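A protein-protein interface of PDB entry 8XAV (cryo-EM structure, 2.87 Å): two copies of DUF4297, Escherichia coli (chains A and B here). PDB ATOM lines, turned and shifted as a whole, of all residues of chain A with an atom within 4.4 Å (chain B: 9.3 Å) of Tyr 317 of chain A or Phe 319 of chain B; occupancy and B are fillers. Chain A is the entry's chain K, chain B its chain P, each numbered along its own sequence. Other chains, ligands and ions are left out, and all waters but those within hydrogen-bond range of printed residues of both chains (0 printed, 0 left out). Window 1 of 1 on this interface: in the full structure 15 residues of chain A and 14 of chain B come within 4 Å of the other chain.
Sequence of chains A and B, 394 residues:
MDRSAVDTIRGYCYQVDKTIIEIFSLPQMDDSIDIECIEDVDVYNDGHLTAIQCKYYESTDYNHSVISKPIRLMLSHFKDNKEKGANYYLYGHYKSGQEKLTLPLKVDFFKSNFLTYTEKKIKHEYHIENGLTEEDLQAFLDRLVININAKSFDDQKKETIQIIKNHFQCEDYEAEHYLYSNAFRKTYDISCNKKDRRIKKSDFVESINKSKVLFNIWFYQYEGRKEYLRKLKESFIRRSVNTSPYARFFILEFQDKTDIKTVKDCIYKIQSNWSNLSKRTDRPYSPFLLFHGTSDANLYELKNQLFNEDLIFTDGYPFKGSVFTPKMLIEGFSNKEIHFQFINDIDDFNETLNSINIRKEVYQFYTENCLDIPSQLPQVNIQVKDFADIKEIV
Tyr 317 of chain A touches just these residues of chain B: Pro 318, Phe 319 and Lys 320.
Of chain A, only Lys 303, Asn 304, Phe 307, Phe 313, Asp 315 and Tyr 317 come within 4 Å of Phe 319 of chain B.
Asn 304 of chain A touches just these residues of chain B: Phe 319 (3.2 Å), Gly 321 (3.4 Å), Ser 322 (3.6 Å) and Val 323 (3.3 Å).
No residue of chain B comes within 4 Å of Gly 316 of chain A.
Pro 318 of chain A touches three residues of chain B.
Printed residues of chain A within 4 Å of Ser 322 of chain B: Asn 304.
Of the printed residues of chain A, Gly 321 of chain B touches Asn 304 (3.4 Å).
Of the printed residues of chain A, Phe 313 of chain B touches Phe 319 (3.8 Å).
Of the printed residues of chain B, Phe 313 of chain A touches Phe 319.
The nearest printed residue of chain A that does not touch Phe 319 of chain B is Pro 318 of chain A (5.3 Å).
The nearest printed residue of chain B that does not touch Asn 344 of chain A is Gly 321 of chain B (6.3 Å).
Of the 16 printed residues of chain B, 12 touch a printed residue of chain A.
Hydrophobic or aromatic side chains of chain B that line the printed part of chain A: Phe 307, Phe 313, Pro 318, Phe 319, Val 323 and Met 328.
Of the 15 printed residues of chain A, 11 touch a printed residue of chain B.
Hydrophobic or aromatic side chains of chain A within 4 Å of the printed part of chain B: Phe 307, Phe 313, Tyr 317, Pro 318, Phe 319 and Val 323.
Among the printed residues, 27 pairs touch across the chains.
Among the printed residues, pairs that only touch across the chains: Lys 303 of chain A with Phe 319 of chain B (3.5 Å), Lys 303 of chain A with Lys 320 of chain B (3.7 Å), Asn 304 of chain A with Phe 319 of chain B (3.2 Å), Asn 304 of chain A with Ser 322 of chain B (3.6 Å), Phe 307 of chain A with Pro 318 of chain B (3.6 Å), Phe 307 of chain A with Phe 319 of chain B (3.6 Å), Phe 307 of chain A with Met 328 of chain B (3.6 Å), Phe 313 of chain A with Phe 319 of chain B (3.7 Å), Asp 315 of chain A with Pro 318 of chain B (3.8 Å), Asp 315 of chain A with Phe 319 of chain B (3.3 Å), Tyr 317 of chain A with Phe 319 of chain B (3.7 Å), Tyr 317 of chain A with Lys 320 of chain B (3.8 Å), Pro 318 of chain A with Phe 307 of chain B (3.7 Å), Pro 318 of chain A with Asp 315 of chain B (3.9 Å), Phe 319 of chain A with Asn 304 of chain B (3.4 Å), Phe 319 of chain A with Phe 307 of chain B (3.5 Å), Phe 319 of chain A with Phe 313 of chain B (3.8 Å), Phe 319 of chain A with Asp 315 of chain B (3.3 Å), Phe 319 of chain A with Tyr 317 of chain B (3.5 Å), Ser 322 of chain A with Asn 304 of chain B (3.7 Å) and Asn 344 of chain A with Lys 320 of chain B (3.6 Å).
OD2 of Asp 315 of chain A lies within salt-bridge range of NZ of Lys 303 of chain A.
The side-chain amino group of Lys 303 of chain A sits at hydrogen-bond distance from the side-chain amide oxygen of Asn 344 of chain A.
N of Tyr 317 of chain A sits at hydrogen-bond distance from OD1 of Asp 315 of chain A.
The side-chain hydroxyl (OH) of Tyr 317 of chain A sits at hydrogen-bond distance from the side-chain carboxylate (OD2) of Asp 348 of chain A, 2.8 Å away.
The backbone NH of Tyr 317 of chain B sits close to the side-chain carboxylate of Asp 315 of chain B, at 3.3 Å.
O of Val 323 of chain B lies within hydrogen-bond range of OG1 of Thr 325 of chain B (2.9 Å).
Phe 307 of chain A touches Pro 318 of chain B, and with the chains exchanged Pro 318 of chain A touches Phe 307 of chain B.
Phe 307 of chain A touches Phe 319 of chain B, and with the chains exchanged Phe 319 of chain A touches Phe 307 of chain B.
Phe 313 of chain A touches Phe 319 of chain B, and with the chains exchanged Phe 319 of chain A touches Phe 313 of chain B.
Tyr 317 of chain A touches Pro 318 of chain B, and with the chains exchanged Pro 318 of chain A touches Tyr 317 of chain B.
Positions printed for both chains: 304, 307, 313, 315, 316, 317, 318, 319, 322, 323 and 324.
Of the 27 pairs that touch across the chains among the printed residues, 20 have their exchanged pair printed and touching as well.
The side-chain amide nitrogen of Asn 304 of chain A sits at hydrogen-bond distance from the backbone carbonyl oxygen of Gly 321 of chain B, 3.4 Å away.
The backbone NH (N) of Val 323 of chain B sits close to the side-chain amide oxygen (OD1) of Asn 304 of chain A, at 3.3 Å.
N of Lys 320 of chain B sits at hydrogen-bond distance from OD2 of Asp 315 of chain A (2.5 Å).
N of Val 323 of chain A lies within hydrogen-bond range of OD1 of Asn 304 of chain B.
The backbone carbonyl oxygen of Tyr 317 of chain A lies close to the backbone carbonyl oxygen of Pro 318 of chain B (3.3 Å).
O of Pro 318 of chain A lies close to O of Tyr 317 of chain B (3.3 Å).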
ATOM      1  N   LYS A 303       6.445  -9.431  25.506  1.00  0.00           N
ATOM      2  CA  LYS A 303       5.575  -8.270  25.675  1.00  0.00           C
ATOM      3  C   LYS A 303       4.343  -8.614  26.502  1.00  0.00           C
ATOM      4  O   LYS A 303       3.871  -7.790  27.295  1.00  0.00           O
ATOM      5  CB  LYS A 303       5.161  -7.717  24.311  1.00  0.00           C
ATOM      6  CG  LYS A 303       6.275  -7.022  23.552  1.00  0.00           C
ATOM      7  CD  LYS A 303       5.947  -6.908  22.073  1.00  0.00           C
ATOM      8  CE  LYS A 303       4.907  -5.831  21.818  1.00  0.00           C
ATOM      9  NZ  LYS A 303       4.990  -5.296  20.432  1.00  0.00           N
ATOM     10  N   ASN A 304       3.804  -9.822  26.324  1.00  0.00           N
ATOM     11  CA  ASN A 304       2.659 -10.246  27.121  1.00  0.00           C
ATOM     12  C   ASN A 304       3.051 -10.469  28.575  1.00  0.00           C
ATOM     13  O   ASN A 304       2.259 -10.199  29.486  1.00  0.00           O
ATOM     14  CB  ASN A 304       2.049 -11.514  26.526  1.00  0.00           C
ATOM     15  CG  ASN A 304       1.252 -11.239  25.269  1.00  0.00           C
ATOM     16  OD1 ASN A 304       0.200 -10.603  25.314  1.00  0.00           O
ATOM     17  ND2 ASN A 304       1.748 -11.719  24.135  1.00  0.00           N
ATOM     18  N   PHE A 307       3.415  -6.923  30.250  1.00  0.00           N
ATOM     19  CA  PHE A 307       2.151  -6.251  30.527  1.00  0.00           C
ATOM     20  C   PHE A 307       1.412  -6.887  31.698  1.00  0.00           C
ATOM     21  O   PHE A 307       0.620  -6.215  32.368  1.00  0.00           O
ATOM     22  CB  PHE A 307       1.274  -6.261  29.275  1.00  0.00           C
ATOM     23  CG  PHE A 307       0.296  -5.125  29.206  1.00  0.00           C
ATOM     24  CD1 PHE A 307      -0.976  -5.253  29.740  1.00  0.00           C
ATOM     25  CD2 PHE A 307       0.647  -3.929  28.602  1.00  0.00           C
ATOM     26  CE1 PHE A 307      -1.879  -4.207  29.677  1.00  0.00           C
ATOM     27  CE2 PHE A 307      -0.251  -2.879  28.533  1.00  0.00           C
ATOM     28  CZ  PHE A 307      -1.515  -3.018  29.072  1.00  0.00           C
ATOM     29  N   PHE A 313       3.461  -0.381  28.667  1.00  0.00           N
ATOM     30  CA  PHE A 313       4.249   0.168  27.574  1.00  0.00           C
ATOM     31  C   PHE A 313       3.339   0.467  26.388  1.00  0.00           C
ATOM     32  O   PHE A 313       2.140   0.168  26.401  1.00  0.00           O
ATOM     33  CB  PHE A 313       5.383  -0.786  27.163  1.00  0.00           C
ATOM     34  CG  PHE A 313       4.918  -2.165  26.775  1.00  0.00           C
ATOM     35  CD1 PHE A 313       4.801  -3.167  27.726  1.00  0.00           C
ATOM     36  CD2 PHE A 313       4.624  -2.468  25.454  1.00  0.00           C
ATOM     37  CE1 PHE A 313       4.380  -4.433  27.372  1.00  0.00           C
ATOM     38  CE2 PHE A 313       4.203  -3.732  25.093  1.00  0.00           C
ATOM     39  CZ  PHE A 313       4.082  -4.717  26.053  1.00  0.00           C
ATOM     40  N   ASP A 315       3.587   0.504  21.836  1.00  0.00           N
ATOM     41  CA  ASP A 315       4.357   0.118  20.660  1.00  0.00           C
ATOM     42  C   ASP A 315       3.944   0.879  19.408  1.00  0.00           C
ATOM     43  O   ASP A 315       4.449   0.579  18.320  1.00  0.00           O
ATOM     44  CB  ASP A 315       4.233  -1.386  20.401  1.00  0.00           C
ATOM     45  CG  ASP A 315       2.798  -1.860  20.387  1.00  0.00           C
ATOM     46  OD1 ASP A 315       1.907  -1.090  20.803  1.00  0.00           O
ATOM     47  OD2 ASP A 315       2.561  -3.000  19.937  1.00  0.00           O
ATOM     48  N   GLY A 316       3.045   1.851  19.526  1.00  0.00           N
ATOM     49  CA  GLY A 316       2.501   2.499  18.353  1.00  0.00           C
ATOM     50  C   GLY A 316       1.357   1.758  17.701  1.00  0.00           C
ATOM     51  O   GLY A 316       0.900   2.174  16.631  1.00  0.00           O
ATOM     52  N   TYR A 317       0.882   0.672  18.312  1.00  0.00           N
ATOM     53  CA  TYR A 317      -0.244  -0.114  17.816  1.00  0.00           C
ATOM     54  C   TYR A 317      -1.285  -0.155  18.927  1.00  0.00           C
ATOM     55  O   TYR A 317      -1.344  -1.120  19.704  1.00  0.00           O
ATOM     56  CB  TYR A 317       0.185  -1.522  17.407  1.00  0.00           C
ATOM     57  CG  TYR A 317       1.261  -1.562  16.346  1.00  0.00           C
ATOM     58  CD1 TYR A 317       0.932  -1.579  14.997  1.00  0.00           C
ATOM     59  CD2 TYR A 317       2.606  -1.594  16.693  1.00  0.00           C
ATOM     60  CE1 TYR A 317       1.912  -1.619  14.022  1.00  0.00           C
ATOM     61  CE2 TYR A 317       3.594  -1.632  15.726  1.00  0.00           C
ATOM     62  CZ  TYR A 317       3.240  -1.646  14.393  1.00  0.00           C
ATOM     63  OH  TYR A 317       4.219  -1.685  13.427  1.00  0.00           O
ATOM     64  N   PRO A 318      -2.122   0.883  19.041  1.00  0.00           N
ATOM     65  CA  PRO A 318      -3.063   0.957  20.169  1.00  0.00           C
ATOM     66  C   PRO A 318      -4.201  -0.048  20.105  1.00  0.00           C
ATOM     67  O   PRO A 318      -4.884  -0.238  21.119  1.00  0.00           O
ATOM     68  CB  PRO A 318      -3.591   2.394  20.086  1.00  0.00           C
ATOM     69  CG  PRO A 318      -3.471   2.742  18.642  1.00  0.00           C
ATOM     70  CD  PRO A 318      -2.219   2.062  18.162  1.00  0.00           C
ATOM     71  N   PHE A 319      -4.432  -0.697  18.966  1.00  0.00           N
ATOM     72  CA  PHE A 319      -5.498  -1.681  18.866  1.00  0.00           C
ATOM     73  C   PHE A 319      -5.107  -2.735  17.839  1.00  0.00           C
ATOM     74  O   PHE A 319      -4.089  -2.620  17.154  1.00  0.00           O
ATOM     75  CB  PHE A 319      -6.845  -1.027  18.518  1.00  0.00           C
ATOM     76  CG  PHE A 319      -6.808  -0.118  17.320  1.00  0.00           C
ATOM     77  CD1 PHE A 319      -7.077  -0.608  16.053  1.00  0.00           C
ATOM     78  CD2 PHE A 319      -6.531   1.232  17.465  1.00  0.00           C
ATOM     79  CE1 PHE A 319      -7.063   0.227  14.951  1.00  0.00           C
ATOM     80  CE2 PHE A 319      -6.504   2.069  16.368  1.00  0.00           C
ATOM     81  CZ  PHE A 319      -6.771   1.566  15.109  1.00  0.00           C
ATOM     82  N   SER A 322      -4.185  -2.126  13.906  1.00  0.00           N
ATOM     83  CA  SER A 322      -3.775  -0.739  13.751  1.00  0.00           C
ATOM     84  C   SER A 322      -2.501  -0.637  12.925  1.00  0.00           C
ATOM     85  O   SER A 322      -1.610  -1.485  13.017  1.00  0.00           O
ATOM     86  CB  SER A 322      -3.549  -0.093  15.118  1.00  0.00           C
ATOM     87  OG  SER A 322      -3.076   1.235  14.982  1.00  0.00           O
ATOM     88  N   VAL A 323      -2.422   0.415  12.108  1.00  0.00           N
ATOM     89  CA  VAL A 323      -1.144   0.772  11.511  1.00  0.00           C
ATOM     90  C   VAL A 323      -0.237   1.370  12.582  1.00  0.00           C
ATOM     91  O   VAL A 323      -0.678   1.753  13.674  1.00  0.00           O
ATOM     92  CB  VAL A 323      -1.335   1.742  10.333  1.00  0.00           C
ATOM     93  CG1 VAL A 323      -2.474   1.273   9.443  1.00  0.00           C
ATOM     94  CG2 VAL A 323      -1.594   3.155  10.836  1.00  0.00           C
ATOM     95  N   PHE A 324       1.053   1.434  12.272  1.00  0.00           N
ATOM     96  CA  PHE A 324       2.020   1.962  13.229  1.00  0.00           C
ATOM     97  C   PHE A 324       1.838   3.469  13.354  1.00  0.00           C
ATOM     98  O   PHE A 324       2.088   4.215  12.402  1.00  0.00           O
ATOM     99  CB  PHE A 324       3.445   1.623  12.808  1.00  0.00           C
ATOM    100  CG  PHE A 324       4.490   2.299  13.646  1.00  0.00           C
ATOM    101  CD1 PHE A 324       4.709   1.899  14.955  1.00  0.00           C
ATOM    102  CD2 PHE A 324       5.248   3.338  13.131  1.00  0.00           C
ATOM    103  CE1 PHE A 324       5.663   2.523  15.734  1.00  0.00           C
ATOM    104  CE2 PHE A 324       6.205   3.964  13.905  1.00  0.00           C
ATOM    105  CZ  PHE A 324       6.413   3.556  15.207  1.00  0.00           C
ATOM    106  N   ASN A 344       8.742  -1.949  17.920  1.00  0.00           N
ATOM    107  CA  ASN A 344       8.555  -3.325  17.473  1.00  0.00           C
ATOM    108  C   ASN A 344       9.640  -3.757  16.490  1.00  0.00           C
ATOM    109  O   ASN A 344      10.372  -4.720  16.744  1.00  0.00           O
ATOM    110  CB  ASN A 344       7.166  -3.483  16.849  1.00  0.00           C
ATOM    111  CG  ASN A 344       6.433  -4.704  17.363  1.00  0.00           C
ATOM    112  OD1 ASN A 344       6.602  -5.104  18.516  1.00  0.00           O
ATOM    113  ND2 ASN A 344       5.612  -5.305  16.511  1.00  0.00           N
ATOM    114  N   ASP A 345       9.759  -3.060  15.364  1.00  0.00           N
ATOM    115  CA  ASP A 345      10.697  -3.438  14.317  1.00  0.00           C
ATOM    116  C   ASP A 345      11.599  -2.261  13.970  1.00  0.00           C
ATOM    117  O   ASP A 345      11.422  -1.141  14.455  1.00  0.00           O
ATOM    118  CB  ASP A 345       9.970  -3.936  13.060  1.00  0.00           C
ATOM    119  CG  ASP A 345       8.750  -4.776  13.384  1.00  0.00           C
ATOM    120  OD1 ASP A 345       7.682  -4.195  13.662  1.00  0.00           O
ATOM    121  OD2 ASP A 345       8.860  -6.020  13.359  1.00  0.00           O
ATOM    122  N   ASP A 348       9.756   0.536  12.155  1.00  0.00           N
ATOM    123  CA  ASP A 348       9.113   1.446  13.093  1.00  0.00           C
ATOM    124  C   ASP A 348      10.115   2.290  13.868  1.00  0.00           C
ATOM    125  O   ASP A 348       9.744   3.349  14.386  1.00  0.00           O
ATOM    126  CB  ASP A 348       8.235   0.662  14.069  1.00  0.00           C
ATOM    127  CG  ASP A 348       7.245  -0.243  13.364  1.00  0.00           C
ATOM    128  OD1 ASP A 348       6.693   0.173  12.325  1.00  0.00           O
ATOM    129  OD2 ASP A 348       7.016  -1.369  13.852  1.00  0.00           O
ATOM    130  N   ASN B 304      -9.313   2.094  12.121  1.00  0.00           N
ATOM    131  CA  ASN B 304      -8.225   3.060  12.012  1.00  0.00           C
ATOM    132  C   ASN B 304      -8.749   4.482  11.851  1.00  0.00           C
ATOM    133  O   ASN B 304      -8.135   5.431  12.352  1.00  0.00           O
ATOM    134  CB  ASN B 304      -7.311   2.689  10.846  1.00  0.00           C
ATOM    135  CG  ASN B 304      -6.160   1.803  11.271  1.00  0.00           C
ATOM    136  OD1 ASN B 304      -5.354   2.179  12.123  1.00  0.00           O
ATOM    137  ND2 ASN B 304      -6.076   0.616  10.683  1.00  0.00           N
ATOM    138  N   PHE B 307      -9.803   6.048  15.321  1.00  0.00           N
ATOM    139  CA  PHE B 307      -8.697   6.529  16.140  1.00  0.00           C
ATOM    140  C   PHE B 307      -8.057   7.775  15.544  1.00  0.00           C
ATOM    141  O   PHE B 307      -7.477   8.584  16.278  1.00  0.00           O
ATOM    142  CB  PHE B 307      -7.655   5.426  16.307  1.00  0.00           C
ATOM    143  CG  PHE B 307      -6.986   5.423  17.649  1.00  0.00           C
ATOM    144  CD1 PHE B 307      -7.594   4.816  18.736  1.00  0.00           C
ATOM    145  CD2 PHE B 307      -5.750   6.022  17.826  1.00  0.00           C
ATOM    146  CE1 PHE B 307      -6.983   4.807  19.976  1.00  0.00           C
ATOM    147  CE2 PHE B 307      -5.133   6.017  19.064  1.00  0.00           C
ATOM    148  CZ  PHE B 307      -5.751   5.409  20.140  1.00  0.00           C
ATOM    149  N   PHE B 313     -10.526   4.656  21.731  1.00  0.00           N
ATOM    150  CA  PHE B 313     -11.247   3.490  22.216  1.00  0.00           C
ATOM    151  C   PHE B 313     -10.236   2.441  22.655  1.00  0.00           C
ATOM    152  O   PHE B 313      -9.022   2.608  22.496  1.00  0.00           O
ATOM    153  CB  PHE B 313     -12.196   2.933  21.145  1.00  0.00           C
ATOM    154  CG  PHE B 313     -11.521   2.609  19.838  1.00  0.00           C
ATOM    155  CD1 PHE B 313     -11.419   3.566  18.842  1.00  0.00           C
ATOM    156  CD2 PHE B 313     -11.007   1.344  19.597  1.00  0.00           C
ATOM    157  CE1 PHE B 313     -10.803   3.279  17.644  1.00  0.00           C
ATOM    158  CE2 PHE B 313     -10.389   1.049  18.399  1.00  0.00           C
ATOM    159  CZ  PHE B 313     -10.289   2.020  17.422  1.00  0.00           C
ATOM    160  N   THR B 314     -10.745   1.347  23.212  1.00  0.00           N
ATOM    161  CA  THR B 314      -9.932   0.196  23.575  1.00  0.00           C
ATOM    162  C   THR B 314     -10.590  -1.061  23.029  1.00  0.00           C
ATOM    163  O   THR B 314     -11.813  -1.126  22.882  1.00  0.00           O
ATOM    164  CB  THR B 314      -9.758   0.074  25.091  1.00  0.00           C
ATOM    165  OG1 THR B 314     -10.965   0.480  25.747  1.00  0.00           O
ATOM    166  CG2 THR B 314      -8.606   0.945  25.569  1.00  0.00           C
ATOM    167  N   ASP B 315      -9.765  -2.064  22.724  1.00  0.00           N
ATOM    168  CA  ASP B 315     -10.286  -3.300  22.156  1.00  0.00           C
ATOM    169  C   ASP B 315      -9.698  -4.546  22.802  1.00  0.00           C
ATOM    170  O   ASP B 315      -9.864  -5.642  22.255  1.00  0.00           O
ATOM    171  CB  ASP B 315     -10.037  -3.344  20.647  1.00  0.00           C
ATOM    172  CG  ASP B 315      -8.569  -3.456  20.304  1.00  0.00           C
ATOM    173  OD1 ASP B 315      -7.737  -2.900  21.052  1.00  0.00           O
ATOM    174  OD2 ASP B 315      -8.245  -4.090  19.278  1.00  0.00           O
ATOM    175  N   GLY B 316      -9.017  -4.420  23.939  1.00  0.00           N
ATOM    176  CA  GLY B 316      -8.422  -5.561  24.596  1.00  0.00           C
ATOM    177  C   GLY B 316      -7.080  -5.995  24.051  1.00  0.00           C
ATOM    178  O   GLY B 316      -6.533  -6.996  24.530  1.00  0.00           O
ATOM    179  N   TYR B 317      -6.532  -5.282  23.067  1.00  0.00           N
ATOM    180  CA  TYR B 317      -5.204  -5.548  22.520  1.00  0.00           C
ATOM    181  C   TYR B 317      -4.399  -4.257  22.623  1.00  0.00           C
ATOM    182  O   TYR B 317      -4.326  -3.480  21.659  1.00  0.00           O
ATOM    183  CB  TYR B 317      -5.268  -6.052  21.079  1.00  0.00           C
ATOM    184  CG  TYR B 317      -6.192  -7.232  20.868  1.00  0.00           C
ATOM    185  CD1 TYR B 317      -7.532  -7.049  20.550  1.00  0.00           C
ATOM    186  CD2 TYR B 317      -5.719  -8.533  20.983  1.00  0.00           C
ATOM    187  CE1 TYR B 317      -8.375  -8.129  20.357  1.00  0.00           C
ATOM    188  CE2 TYR B 317      -6.553  -9.618  20.790  1.00  0.00           C
ATOM    189  CZ  TYR B 317      -7.879  -9.410  20.478  1.00  0.00           C
ATOM    190  OH  TYR B 317      -8.713 -10.488  20.286  1.00  0.00           O
ATOM    191  N   PRO B 318      -3.788  -3.993  23.782  1.00  0.00           N
ATOM    192  CA  PRO B 318      -3.046  -2.733  23.952  1.00  0.00           C
ATOM    193  C   PRO B 318      -1.759  -2.662  23.149  1.00  0.00           C
ATOM    194  O   PRO B 318      -1.218  -1.561  22.984  1.00  0.00           O
ATOM    195  CB  PRO B 318      -2.764  -2.695  25.459  1.00  0.00           C
ATOM    196  CG  PRO B 318      -2.744  -4.133  25.861  1.00  0.00           C
ATOM    197  CD  PRO B 318      -3.776  -4.812  25.006  1.00  0.00           C
ATOM    198  N   PHE B 319      -1.253  -3.785  22.648  1.00  0.00           N
ATOM    199  CA  PHE B 319      -0.034  -3.795  21.855  1.00  0.00           C
ATOM    200  C   PHE B 319      -0.157  -4.853  20.766  1.00  0.00           C
ATOM    201  O   PHE B 319      -1.100  -5.648  20.744  1.00  0.00           O
ATOM    202  CB  PHE B 319       1.211  -4.029  22.729  1.00  0.00           C
ATOM    203  CG  PHE B 319       1.131  -5.249  23.608  1.00  0.00           C
ATOM    204  CD1 PHE B 319       0.617  -5.161  24.893  1.00  0.00           C
ATOM    205  CD2 PHE B 319       1.607  -6.473  23.165  1.00  0.00           C
ATOM    206  CE1 PHE B 319       0.552  -6.276  25.706  1.00  0.00           C
ATOM    207  CE2 PHE B 319       1.550  -7.590  23.977  1.00  0.00           C
ATOM    208  CZ  PHE B 319       1.020  -7.491  25.248  1.00  0.00           C
ATOM    209  N   LYS B 320       0.803  -4.843  19.845  1.00  0.00           N
ATOM    210  CA  LYS B 320       0.784  -5.780  18.731  1.00  0.00           C
ATOM    211  C   LYS B 320       1.119  -7.189  19.206  1.00  0.00           C
ATOM    212  O   LYS B 320       2.007  -7.387  20.039  1.00  0.00           O
ATOM    213  CB  LYS B 320       1.771  -5.339  17.651  1.00  0.00           C
ATOM    214  CG  LYS B 320       1.598  -6.051  16.320  1.00  0.00           C
ATOM    215  CD  LYS B 320       2.300  -5.304  15.197  1.00  0.00           C
ATOM    216  CE  LYS B 320       2.050  -5.968  13.854  1.00  0.00           C
ATOM    217  NZ  LYS B 320       2.536  -5.129  12.725  1.00  0.00           N
ATOM    218  N   GLY B 321       0.401  -8.171  18.665  1.00  0.00           N
ATOM    219  CA  GLY B 321       0.620  -9.552  19.050  1.00  0.00           C
ATOM    220  C   GLY B 321       0.145  -9.890  20.443  1.00  0.00           C
ATOM    221  O   GLY B 321       0.665 -10.826  21.058  1.00  0.00           O
ATOM    222  N   SER B 322      -0.829  -9.150  20.962  1.00  0.00           N
ATOM    223  CA  SER B 322      -1.306  -9.340  22.321  1.00  0.00           C
ATOM    224  C   SER B 322      -2.435 -10.358  22.372  1.00  0.00           C
ATOM    225  O   SER B 322      -3.230 -10.489  21.437  1.00  0.00           O
ATOM    226  CB  SER B 322      -1.795  -8.016  22.914  1.00  0.00           C
ATOM    227  OG  SER B 322      -2.299  -8.199  24.225  1.00  0.00           O
ATOM    228  N   VAL B 323      -2.483 -11.097  23.480  1.00  0.00           N
ATOM    229  CA  VAL B 323      -3.682 -11.845  23.824  1.00  0.00           C
ATOM    230  C   VAL B 323      -4.742 -10.846  24.275  1.00  0.00           C
ATOM    231  O   VAL B 323      -4.426  -9.788  24.841  1.00  0.00           O
ATOM    232  CB  VAL B 323      -3.359 -12.890  24.914  1.00  0.00           C
ATOM    233  CG1 VAL B 323      -2.536 -12.267  26.031  1.00  0.00           C
ATOM    234  CG2 VAL B 323      -4.607 -13.601  25.461  1.00  0.00           C
ATOM    235  N   PHE B 324      -6.005 -11.152  23.959  1.00  0.00           N
ATOM    236  CA  PHE B 324      -7.139 -10.314  24.337  1.00  0.00           C
ATOM    237  C   PHE B 324      -7.155 -10.060  25.838  1.00  0.00           C
ATOM    238  O   PHE B 324      -7.290 -10.992  26.638  1.00  0.00           O
ATOM    239  CB  PHE B 324      -8.439 -10.981  23.893  1.00  0.00           C
ATOM    240  CG  PHE B 324      -9.663 -10.165  24.170  1.00  0.00           C
ATOM    241  CD1 PHE B 324      -9.760  -8.859  23.719  1.00  0.00           C
ATOM    242  CD2 PHE B 324     -10.714 -10.701  24.895  1.00  0.00           C
ATOM    243  CE1 PHE B 324     -10.892  -8.106  23.975  1.00  0.00           C
ATOM    244  CE2 PHE B 324     -11.843  -9.955  25.157  1.00  0.00           C
ATOM    245  CZ  PHE B 324     -11.933  -8.654  24.696  1.00  0.00           C
ATOM    246  N   THR B 325      -7.014  -8.790  26.211  1.00  0.00           N
ATOM    247  CA  THR B 325      -6.877  -8.388  27.604  1.00  0.00           C
ATOM    248  C   THR B 325      -8.193  -7.775  28.059  1.00  0.00           C
ATOM    249  O   THR B 325      -8.494  -6.621  27.713  1.00  0.00           O
ATOM    250  CB  THR B 325      -5.737  -7.378  27.759  1.00  0.00           C
ATOM    251  OG1 THR B 325      -4.591  -7.813  27.016  1.00  0.00           O
ATOM    252  CG2 THR B 325      -5.352  -7.236  29.215  1.00  0.00           C
ATOM    253  N   MET B 328      -8.300  -4.298  30.072  1.00  0.00           N
ATOM    254  CA  MET B 328      -8.219  -3.073  29.275  1.00  0.00           C
ATOM    255  C   MET B 328      -9.595  -2.516  28.931  1.00  0.00           C
ATOM    256  O   MET B 328      -9.758  -1.295  28.828  1.00  0.00           O
ATOM    257  CB  MET B 328      -7.417  -3.323  27.996  1.00  0.00           C
ATOM    258  CG  MET B 328      -5.870  -3.226  28.041  1.00  0.00           C
ATOM    259  SD  MET B 328      -4.962  -1.899  28.908  1.00  0.00           S
ATOM    260  CE  MET B 328      -5.088  -2.245  30.662  1.00  0.00           C
